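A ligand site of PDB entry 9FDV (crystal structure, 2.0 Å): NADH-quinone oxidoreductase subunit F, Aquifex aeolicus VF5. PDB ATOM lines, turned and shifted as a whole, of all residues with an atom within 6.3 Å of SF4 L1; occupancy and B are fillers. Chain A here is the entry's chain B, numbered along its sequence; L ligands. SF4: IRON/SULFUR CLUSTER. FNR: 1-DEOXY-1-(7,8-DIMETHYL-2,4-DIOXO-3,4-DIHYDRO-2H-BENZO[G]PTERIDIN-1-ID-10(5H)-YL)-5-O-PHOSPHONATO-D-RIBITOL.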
ATOM      1  N   ILE A 181       1.889  15.161 -10.338  1.00  0.00           N
ATOM      2  CA  ILE A 181       2.649  15.755 -11.416  1.00  0.00           C
ATOM      3  C   ILE A 181       2.622  14.854 -12.654  1.00  0.00           C
ATOM      4  O   ILE A 181       2.814  15.340 -13.764  1.00  0.00           O
ATOM      5  CB  ILE A 181       4.086  16.099 -10.988  1.00  0.00           C
ATOM      6  CG1 ILE A 181       4.802  16.978 -11.987  1.00  0.00           C
ATOM      7  CG2 ILE A 181       4.895  14.831 -10.725  1.00  0.00           C
ATOM      8  CD1 ILE A 181       4.057  18.253 -12.332  1.00  0.00           C
ATOM      9  N   HIS A 198       9.052  13.473 -13.988  1.00  0.00           N
ATOM     10  CA  HIS A 198       9.677  14.788 -13.979  1.00  0.00           C
ATOM     11  C   HIS A 198       9.291  15.475 -15.275  1.00  0.00           C
ATOM     12  O   HIS A 198       9.639  15.003 -16.360  1.00  0.00           O
ATOM     13  CB  HIS A 198      11.196  14.661 -13.871  1.00  0.00           C
ATOM     14  CG  HIS A 198      11.724  14.497 -12.503  1.00  0.00           C
ATOM     15  ND1 HIS A 198      13.041  14.139 -12.297  1.00  0.00           N
ATOM     16  CD2 HIS A 198      11.216  14.714 -11.280  1.00  0.00           C
ATOM     17  CE1 HIS A 198      13.295  14.104 -11.002  1.00  0.00           C
ATOM     18  NE2 HIS A 198      12.199  14.453 -10.364  1.00  0.00           N
ATOM     19  N   PRO A 199       8.547  16.600 -15.240  1.00  0.00           N
ATOM     20  CA  PRO A 199       8.262  17.321 -16.477  1.00  0.00           C
ATOM     21  C   PRO A 199       9.533  17.656 -17.252  1.00  0.00           C
ATOM     22  O   PRO A 199      10.617  17.814 -16.689  1.00  0.00           O
ATOM     23  CB  PRO A 199       7.488  18.555 -15.988  1.00  0.00           C
ATOM     24  CG  PRO A 199       6.845  18.104 -14.690  1.00  0.00           C
ATOM     25  CD  PRO A 199       7.881  17.179 -14.063  1.00  0.00           C
ATOM     26  N   ARG A 200       9.381  17.702 -18.579  1.00  0.00           N
ATOM     27  CA  ARG A 200      10.460  18.096 -19.467  1.00  0.00           C
ATOM     28  C   ARG A 200      10.275  19.561 -19.856  1.00  0.00           C
ATOM     29  O   ARG A 200       9.152  20.045 -19.928  1.00  0.00           O
ATOM     30  CB  ARG A 200      10.445  17.314 -20.786  1.00  0.00           C
ATOM     31  CG  ARG A 200      10.391  15.803 -20.654  1.00  0.00           C
ATOM     32  CD  ARG A 200      10.235  15.196 -22.052  1.00  0.00           C
ATOM     33  NE  ARG A 200      10.333  13.741 -22.048  1.00  0.00           N
ATOM     34  CZ  ARG A 200      10.074  12.927 -23.064  1.00  0.00           C
ATOM     35  NH1 ARG A 200       9.560  13.394 -24.195  1.00  0.00           N
ATOM     36  NH2 ARG A 200      10.319  11.631 -22.934  1.00  0.00           N
ATOM     37  N   GLU A 345       3.124  18.061  -3.910  1.00  0.00           N
ATOM     38  CA  GLU A 345       3.108  17.599  -5.296  1.00  0.00           C
ATOM     39  C   GLU A 345       4.227  18.196  -6.163  1.00  0.00           C
ATOM     40  O   GLU A 345       4.534  17.630  -7.212  1.00  0.00           O
ATOM     41  CB  GLU A 345       1.718  17.799  -5.906  1.00  0.00           C
ATOM     42  CG  GLU A 345       0.627  17.024  -5.173  1.00  0.00           C
ATOM     43  CD  GLU A 345       0.822  15.525  -5.097  1.00  0.00           C
ATOM     44  OE1 GLU A 345       1.635  14.958  -5.891  1.00  0.00           O
ATOM     45  OE2 GLU A 345       0.153  14.903  -4.218  1.00  0.00           O
ATOM     46  N   THR A 346       4.890  19.285  -5.751  1.00  0.00           N
ATOM     47  CA  THR A 346       6.026  19.771  -6.535  1.00  0.00           C
ATOM     48  C   THR A 346       7.019  18.623  -6.698  1.00  0.00           C
ATOM     49  O   THR A 346       7.304  17.929  -5.734  1.00  0.00           O
ATOM     50  CB  THR A 346       6.681  21.014  -5.924  1.00  0.00           C
ATOM     51  OG1 THR A 346       7.874  21.285  -6.662  1.00  0.00           O
ATOM     52  CG2 THR A 346       7.050  20.852  -4.450  1.00  0.00           C
ATOM     53  N   CYS A 347       7.541  18.430  -7.926  1.00  0.00           N
ATOM     54  CA  CYS A 347       8.518  17.373  -8.186  1.00  0.00           C
ATOM     55  C   CYS A 347       9.942  17.787  -7.777  1.00  0.00           C
ATOM     56  O   CYS A 347      10.829  16.953  -7.707  1.00  0.00           O
ATOM     57  CB  CYS A 347       8.462  16.937  -9.650  1.00  0.00           C
ATOM     58  SG  CYS A 347       9.276  18.090 -10.797  1.00  0.00           S
ATOM     59  N   GLY A 348      10.171  19.104  -7.592  1.00  0.00           N
ATOM     60  CA  GLY A 348      11.393  19.605  -7.007  1.00  0.00           C
ATOM     61  C   GLY A 348      12.487  19.988  -8.009  1.00  0.00           C
ATOM     62  O   GLY A 348      13.565  20.391  -7.567  1.00  0.00           O
ATOM     63  N   GLN A 349      12.237  19.884  -9.331  1.00  0.00           N
ATOM     64  CA  GLN A 349      13.279  20.116 -10.325  1.00  0.00           C
ATOM     65  C   GLN A 349      13.708  21.583 -10.378  1.00  0.00           C
ATOM     66  O   GLN A 349      14.864  21.887 -10.703  1.00  0.00           O
ATOM     67  CB  GLN A 349      12.895  19.829 -11.777  1.00  0.00           C
ATOM     68  CG  GLN A 349      12.604  18.380 -12.127  1.00  0.00           C
ATOM     69  CD  GLN A 349      12.298  18.218 -13.596  1.00  0.00           C
ATOM     70  OE1 GLN A 349      11.138  18.245 -14.059  1.00  0.00           O
ATOM     71  NE2 GLN A 349      13.359  18.096 -14.377  1.00  0.00           N
ATOM     72  N   CYS A 350      12.737  22.477 -10.183  1.00  0.00           N
ATOM     73  CA  CYS A 350      12.933  23.908 -10.313  1.00  0.00           C
ATOM     74  C   CYS A 350      13.027  24.500  -8.920  1.00  0.00           C
ATOM     75  O   CYS A 350      12.209  24.167  -8.055  1.00  0.00           O
ATOM     76  CB  CYS A 350      11.790  24.567 -11.074  1.00  0.00           C
ATOM     77  SG  CYS A 350      11.274  23.674 -12.561  1.00  0.00           S
ATOM     78  N   THR A 351      14.004  25.393  -8.698  1.00  0.00           N
ATOM     79  CA  THR A 351      14.290  25.814  -7.327  1.00  0.00           C
ATOM     80  C   THR A 351      13.141  26.630  -6.736  1.00  0.00           C
ATOM     81  O   THR A 351      12.687  26.324  -5.642  1.00  0.00           O
ATOM     82  CB  THR A 351      15.650  26.523  -7.244  1.00  0.00           C
ATOM     83  OG1 THR A 351      16.590  25.448  -7.299  1.00  0.00           O
ATOM     84  CG2 THR A 351      15.870  27.243  -5.932  1.00  0.00           C
ATOM     85  N   CYS A 353       9.954  26.729  -7.314  1.00  0.00           N
ATOM     86  CA  CYS A 353       8.844  25.820  -7.093  1.00  0.00           C
ATOM     87  C   CYS A 353       9.120  24.863  -5.918  1.00  0.00           C
ATOM     88  O   CYS A 353       8.275  24.722  -5.029  1.00  0.00           O
ATOM     89  CB  CYS A 353       8.516  25.052  -8.371  1.00  0.00           C
ATOM     90  SG  CYS A 353       7.118  23.905  -8.206  1.00  0.00           S
ATOM     91  N   ARG A 354      10.295  24.241  -5.907  1.00  0.00           N
ATOM     92  CA  ARG A 354      10.661  23.312  -4.845  1.00  0.00           C
ATOM     93  C   ARG A 354      10.582  23.992  -3.467  1.00  0.00           C
ATOM     94  O   ARG A 354       9.942  23.476  -2.548  1.00  0.00           O
ATOM     95  CB  ARG A 354      12.091  22.801  -5.018  1.00  0.00           C
ATOM     96  CG  ARG A 354      12.569  21.796  -3.976  1.00  0.00           C
ATOM     97  CD  ARG A 354      13.965  21.255  -4.296  1.00  0.00           C
ATOM     98  NE  ARG A 354      14.978  22.318  -4.271  1.00  0.00           N
ATOM     99  CZ  ARG A 354      15.590  22.828  -5.322  1.00  0.00           C
ATOM    100  NH1 ARG A 354      15.308  22.373  -6.543  1.00  0.00           N
ATOM    101  NH2 ARG A 354      16.499  23.793  -5.155  1.00  0.00           N
ATOM    102  N   CYS A 357       6.829  26.099  -2.900  1.00  0.00           N
ATOM    103  CA  CYS A 357       5.654  25.332  -2.498  1.00  0.00           C
ATOM    104  C   CYS A 357       5.793  24.914  -1.033  1.00  0.00           C
ATOM    105  O   CYS A 357       4.814  24.977  -0.273  1.00  0.00           O
ATOM    106  CB  CYS A 357       5.411  24.105  -3.375  1.00  0.00           C
ATOM    107  SG  CYS A 357       4.921  24.496  -5.073  1.00  0.00           S
ATOM    108  N   ILE A 387       6.908  31.667  -6.648  1.00  0.00           N
ATOM    109  CA  ILE A 387       6.980  30.239  -6.908  1.00  0.00           C
ATOM    110  C   ILE A 387       7.237  30.013  -8.403  1.00  0.00           C
ATOM    111  O   ILE A 387       7.934  29.057  -8.777  1.00  0.00           O
ATOM    112  CB  ILE A 387       5.696  29.523  -6.433  1.00  0.00           C
ATOM    113  CG1 ILE A 387       5.353  29.922  -4.981  1.00  0.00           C
ATOM    114  CG2 ILE A 387       5.790  28.012  -6.622  1.00  0.00           C
ATOM    115  CD1 ILE A 387       4.087  29.283  -4.431  1.00  0.00           C
ATOM    116  N   THR A 390      11.366  30.622 -13.298  1.00  0.00           N
ATOM    117  CA  THR A 390      12.193  29.546 -13.838  1.00  0.00           C
ATOM    118  C   THR A 390      11.428  28.227 -13.959  1.00  0.00           C
ATOM    119  O   THR A 390      12.004  27.257 -14.429  1.00  0.00           O
ATOM    120  CB  THR A 390      13.508  29.350 -13.070  1.00  0.00           C
ATOM    121  OG1 THR A 390      13.260  28.558 -11.912  1.00  0.00           O
ATOM    122  CG2 THR A 390      14.172  30.664 -12.686  1.00  0.00           C
ATOM    123  N   SER A 391      10.131  28.186 -13.578  1.00  0.00           N
ATOM    124  CA  SER A 391       9.343  26.964 -13.635  1.00  0.00           C
ATOM    125  C   SER A 391       9.198  26.468 -15.072  1.00  0.00           C
ATOM    126  O   SER A 391       9.014  27.241 -16.000  1.00  0.00           O
ATOM    127  CB  SER A 391       7.990  27.162 -13.001  1.00  0.00           C
ATOM    128  OG  SER A 391       7.257  28.200 -13.639  1.00  0.00           O
ATOM    129  N   ILE A 392       9.257  25.141 -15.265  1.00  0.00           N
ATOM    130  CA  ILE A 392       9.175  24.569 -16.595  1.00  0.00           C
ATOM    131  C   ILE A 392       7.860  23.833 -16.790  1.00  0.00           C
ATOM    132  O   ILE A 392       7.667  23.239 -17.842  1.00  0.00           O
ATOM    133  CB  ILE A 392      10.398  23.663 -16.883  1.00  0.00           C
ATOM    134  CG1 ILE A 392      10.495  22.439 -15.952  1.00  0.00           C
ATOM    135  CG2 ILE A 392      11.702  24.476 -16.866  1.00  0.00           C
ATOM    136  CD1 ILE A 392      11.691  21.533 -16.232  1.00  0.00           C
ATOM    137  N   CYS A 393       6.961  23.855 -15.801  1.00  0.00           N
ATOM    138  CA  CYS A 393       5.632  23.282 -16.001  1.00  0.00           C
ATOM    139  C   CYS A 393       4.578  24.152 -15.301  1.00  0.00           C
ATOM    140  O   CYS A 393       4.930  25.093 -14.579  1.00  0.00           O
ATOM    141  CB  CYS A 393       5.569  21.801 -15.618  1.00  0.00           C
ATOM    142  SG  CYS A 393       4.997  21.442 -13.922  1.00  0.00           S
ATOM    143  N   GLY A 394       3.309  23.811 -15.534  1.00  0.00           N
ATOM    144  CA  GLY A 394       2.175  24.603 -15.076  1.00  0.00           C
ATOM    145  C   GLY A 394       2.005  24.643 -13.558  1.00  0.00           C
ATOM    146  O   GLY A 394       1.367  25.556 -13.045  1.00  0.00           O
ATOM    147  N   LEU A 395       2.554  23.669 -12.823  1.00  0.00           N
ATOM    148  CA  LEU A 395       2.346  23.584 -11.392  1.00  0.00           C
ATOM    149  C   LEU A 395       3.001  24.789 -10.710  1.00  0.00           C
ATOM    150  O   LEU A 395       2.378  25.429  -9.861  1.00  0.00           O
ATOM    151  CB  LEU A 395       2.897  22.285 -10.822  1.00  0.00           C
ATOM    152  CG  LEU A 395       2.574  22.002  -9.345  1.00  0.00           C
ATOM    153  CD1 LEU A 395       2.454  20.507  -9.095  1.00  0.00           C
ATOM    154  CD2 LEU A 395       3.599  22.613  -8.385  1.00  0.00           C
ATOM    155  N   GLY A 396       4.265  25.039 -11.041  1.00  0.00           N
ATOM    156  CA  GLY A 396       4.985  26.179 -10.477  1.00  0.00           C
ATOM    157  C   GLY A 396       4.317  27.494 -10.858  1.00  0.00           C
ATOM    158  O   GLY A 396       4.269  28.429 -10.062  1.00  0.00           O
ATOM    159  N   ALA A 397       3.773  27.554 -12.065  1.00  0.00           N
ATOM    160  CA  ALA A 397       3.109  28.756 -12.565  1.00  0.00           C
ATOM    161  C   ALA A 397       1.839  29.074 -11.773  1.00  0.00           C
ATOM    162  O   ALA A 397       1.447  30.232 -11.754  1.00  0.00           O
ATOM    163  CB  ALA A 397       2.827  28.586 -14.054  1.00  0.00           C
HETATM  164 FE1  SF4 L   1       8.485  20.185 -11.022  1.00  0.00          FE
HETATM  165 FE2  SF4 L   1       7.457  22.599 -10.061  1.00  0.00          FE
HETATM  166 FE3  SF4 L   1       6.808  21.699 -12.536  1.00  0.00          FE
HETATM  167 FE4  SF4 L   1       9.360  22.568 -11.992  1.00  0.00          FE
HETATM  168  S1  SF4 L   1       7.388  23.850 -11.923  1.00  0.00           S
HETATM  169  S2  SF4 L   1       8.800  20.755 -13.226  1.00  0.00           S
HETATM  170  S3  SF4 L   1       9.617  21.814  -9.873  1.00  0.00           S
HETATM  171  S4  SF4 L   1       6.291  20.671 -10.567  1.00  0.00           S
HETATM  172  C9A FNR L   2      -2.067  18.580 -16.030  1.00  0.00           C
HETATM  173  N10 FNR L   2      -2.933  18.114 -17.056  1.00  0.00           N
HETATM  174  CAA FNR L   2      -3.779  17.053 -16.795  1.00  0.00           C
HETATM  175  N1  FNR L   2      -4.546  16.564 -17.812  1.00  0.00           N
HETATM  176  C2  FNR L   2      -5.346  15.462 -17.682  1.00  0.00           C
HETATM  177  O2  FNR L   2      -5.986  14.995 -18.630  1.00  0.00           O
HETATM  178  N3  FNR L   2      -5.383  14.903 -16.435  1.00  0.00           N
HETATM  179  C4  FNR L   2      -4.675  15.310 -15.322  1.00  0.00           C
HETATM  180  O4  FNR L   2      -4.829  14.721 -14.251  1.00  0.00           O
HETATM  181  C4A FNR L   2      -3.816  16.432 -15.568  1.00  0.00           C
HETATM  182  N5  FNR L   2      -2.987  16.863 -14.585  1.00  0.00           N
HETATM  183  C5A FNR L   2      -2.081  17.906 -14.799  1.00  0.00           C
HETATM  184  C6  FNR L   2      -1.211  18.295 -13.780  1.00  0.00           C
HETATM  185  C7  FNR L   2      -0.342  19.371 -13.970  1.00  0.00           C
HETATM  186  C7M FNR L   2       0.557  19.779 -12.839  1.00  0.00           C
HETATM  187  C8  FNR L   2      -0.343  20.054 -15.202  1.00  0.00           C
HETATM  188  C8M FNR L   2       0.469  21.311 -15.394  1.00  0.00           C
HETATM  189  C9  FNR L   2      -1.204  19.644 -16.217  1.00  0.00           C
HETATM  190  C1' FNR L   2      -2.923  18.732 -18.390  1.00  0.00           C
HETATM  191  C2' FNR L   2      -2.064  17.877 -19.325  1.00  0.00           C
HETATM  192  O2' FNR L   2      -0.684  18.275 -19.260  1.00  0.00           O
HETATM  193  C3' FNR L   2      -2.536  18.036 -20.772  1.00  0.00           C
HETATM  194  O3' FNR L   2      -2.752  19.411 -21.067  1.00  0.00           O
HETATM  195  C4' FNR L   2      -3.792  17.234 -21.102  1.00  0.00           C
HETATM  196  O4' FNR L   2      -3.711  15.908 -20.580  1.00  0.00           O
HETATM  197  C5' FNR L   2      -4.030  17.226 -22.597  1.00  0.00           C
HETATM  198  O5' FNR L   2      -5.310  16.654 -22.921  1.00  0.00           O
HETATM  199  P   FNR L   2      -6.513  17.645 -23.378  1.00  0.00           P
HETATM  200  O1P FNR L   2      -6.091  18.576 -24.488  1.00  0.00           O
HETATM  201  O2P FNR L   2      -6.988  18.392 -22.169  1.00  0.00           O
HETATM  202  O3P FNR L   2      -7.525  16.599 -23.840  1.00  0.00           O
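The backbone NH of Gly 348 sits close to a sulfur (S3) of SF4 L1 (3.6 Å).
SG of Cys 353 is bound to FE2 of SF4 L1 (2.3 Å).
A sulfur (S2) of SF4 L1 lies close to the side-chain amide oxygen (OE1) of Gln 349.
A sulfur (S4) of SF4 L1 lies close to the backbone NH of Cys 347, at 3.7 Å.
An iron atom (FE1) of SF4 L1 is bound by the side-chain sulfur of Cys 347 (2.3 Å).
N of Gln 349 sits close to S3 of SF4 L1.
A sulfur (S1) of SF4 L1 lies close to the backbone NH (N) of Gly 396, at 3.5 Å.
The side-chain hydroxyl (OG1) of Thr 346 lies close to a sulfur (S3) of SF4 L1, at 3.7 Å.
The side-chain sulfur of Cys 393 is bound to an iron atom (FE3) of SF4 L1 (2.3 Å).
An iron atom (FE4) of SF4 L1 is bound by the side-chain sulfur (SG) of Cys 350, 2.3 Å away.
S3 of SF4 L1 lies close to N of Cys 350, at 3.2 Å.
The backbone carbonyl oxygen (O) of Cys 353 is in hydrogen-bond range of the side-chain sulfur (SG) of Cys 357 (3.4 Å).
The backbone carbonyl oxygen (O) of Gly 348 sits at hydrogen-bond distance from the guanidinium group (NH1) of Arg 354 (2.8 Å).
N of Cys 353 lies within hydrogen-bond range of O of Ile 387.
N of Gly 348 lies within hydrogen-bond range of OG1 of Thr 346 (3.3 Å).
OE1 of Gln 349 sits close to SG of Cys 347, at 3.8 Å.
SG of Cys 353 sits close to OG1 of Thr 346 (3.1 Å).
The side-chain sulfur (SG) of Cys 393 lies close to the backbone NH (N) of Leu 395, 3.5 Å away.
The side-chain sulfur (SG) of Cys 350 lies close to the backbone NH (N) of Ile 392.
CD1 of Ile 181 touches S4 of SF4 L1, at 3.7 Å.
CG of Pro 199 touches S2 of SF4 L1, 3.6 Å away.
Ser 391 touches SF4 L1 (CB to S1, 3.5 Å).
Ile 392 touches SF4 L1 (CG1 to S2, 3.6 Å).
Leu 395 touches SF4 L1.
The nearest printed residue that does not touch SF4 L1 is Arg 354 (4.7 Å).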
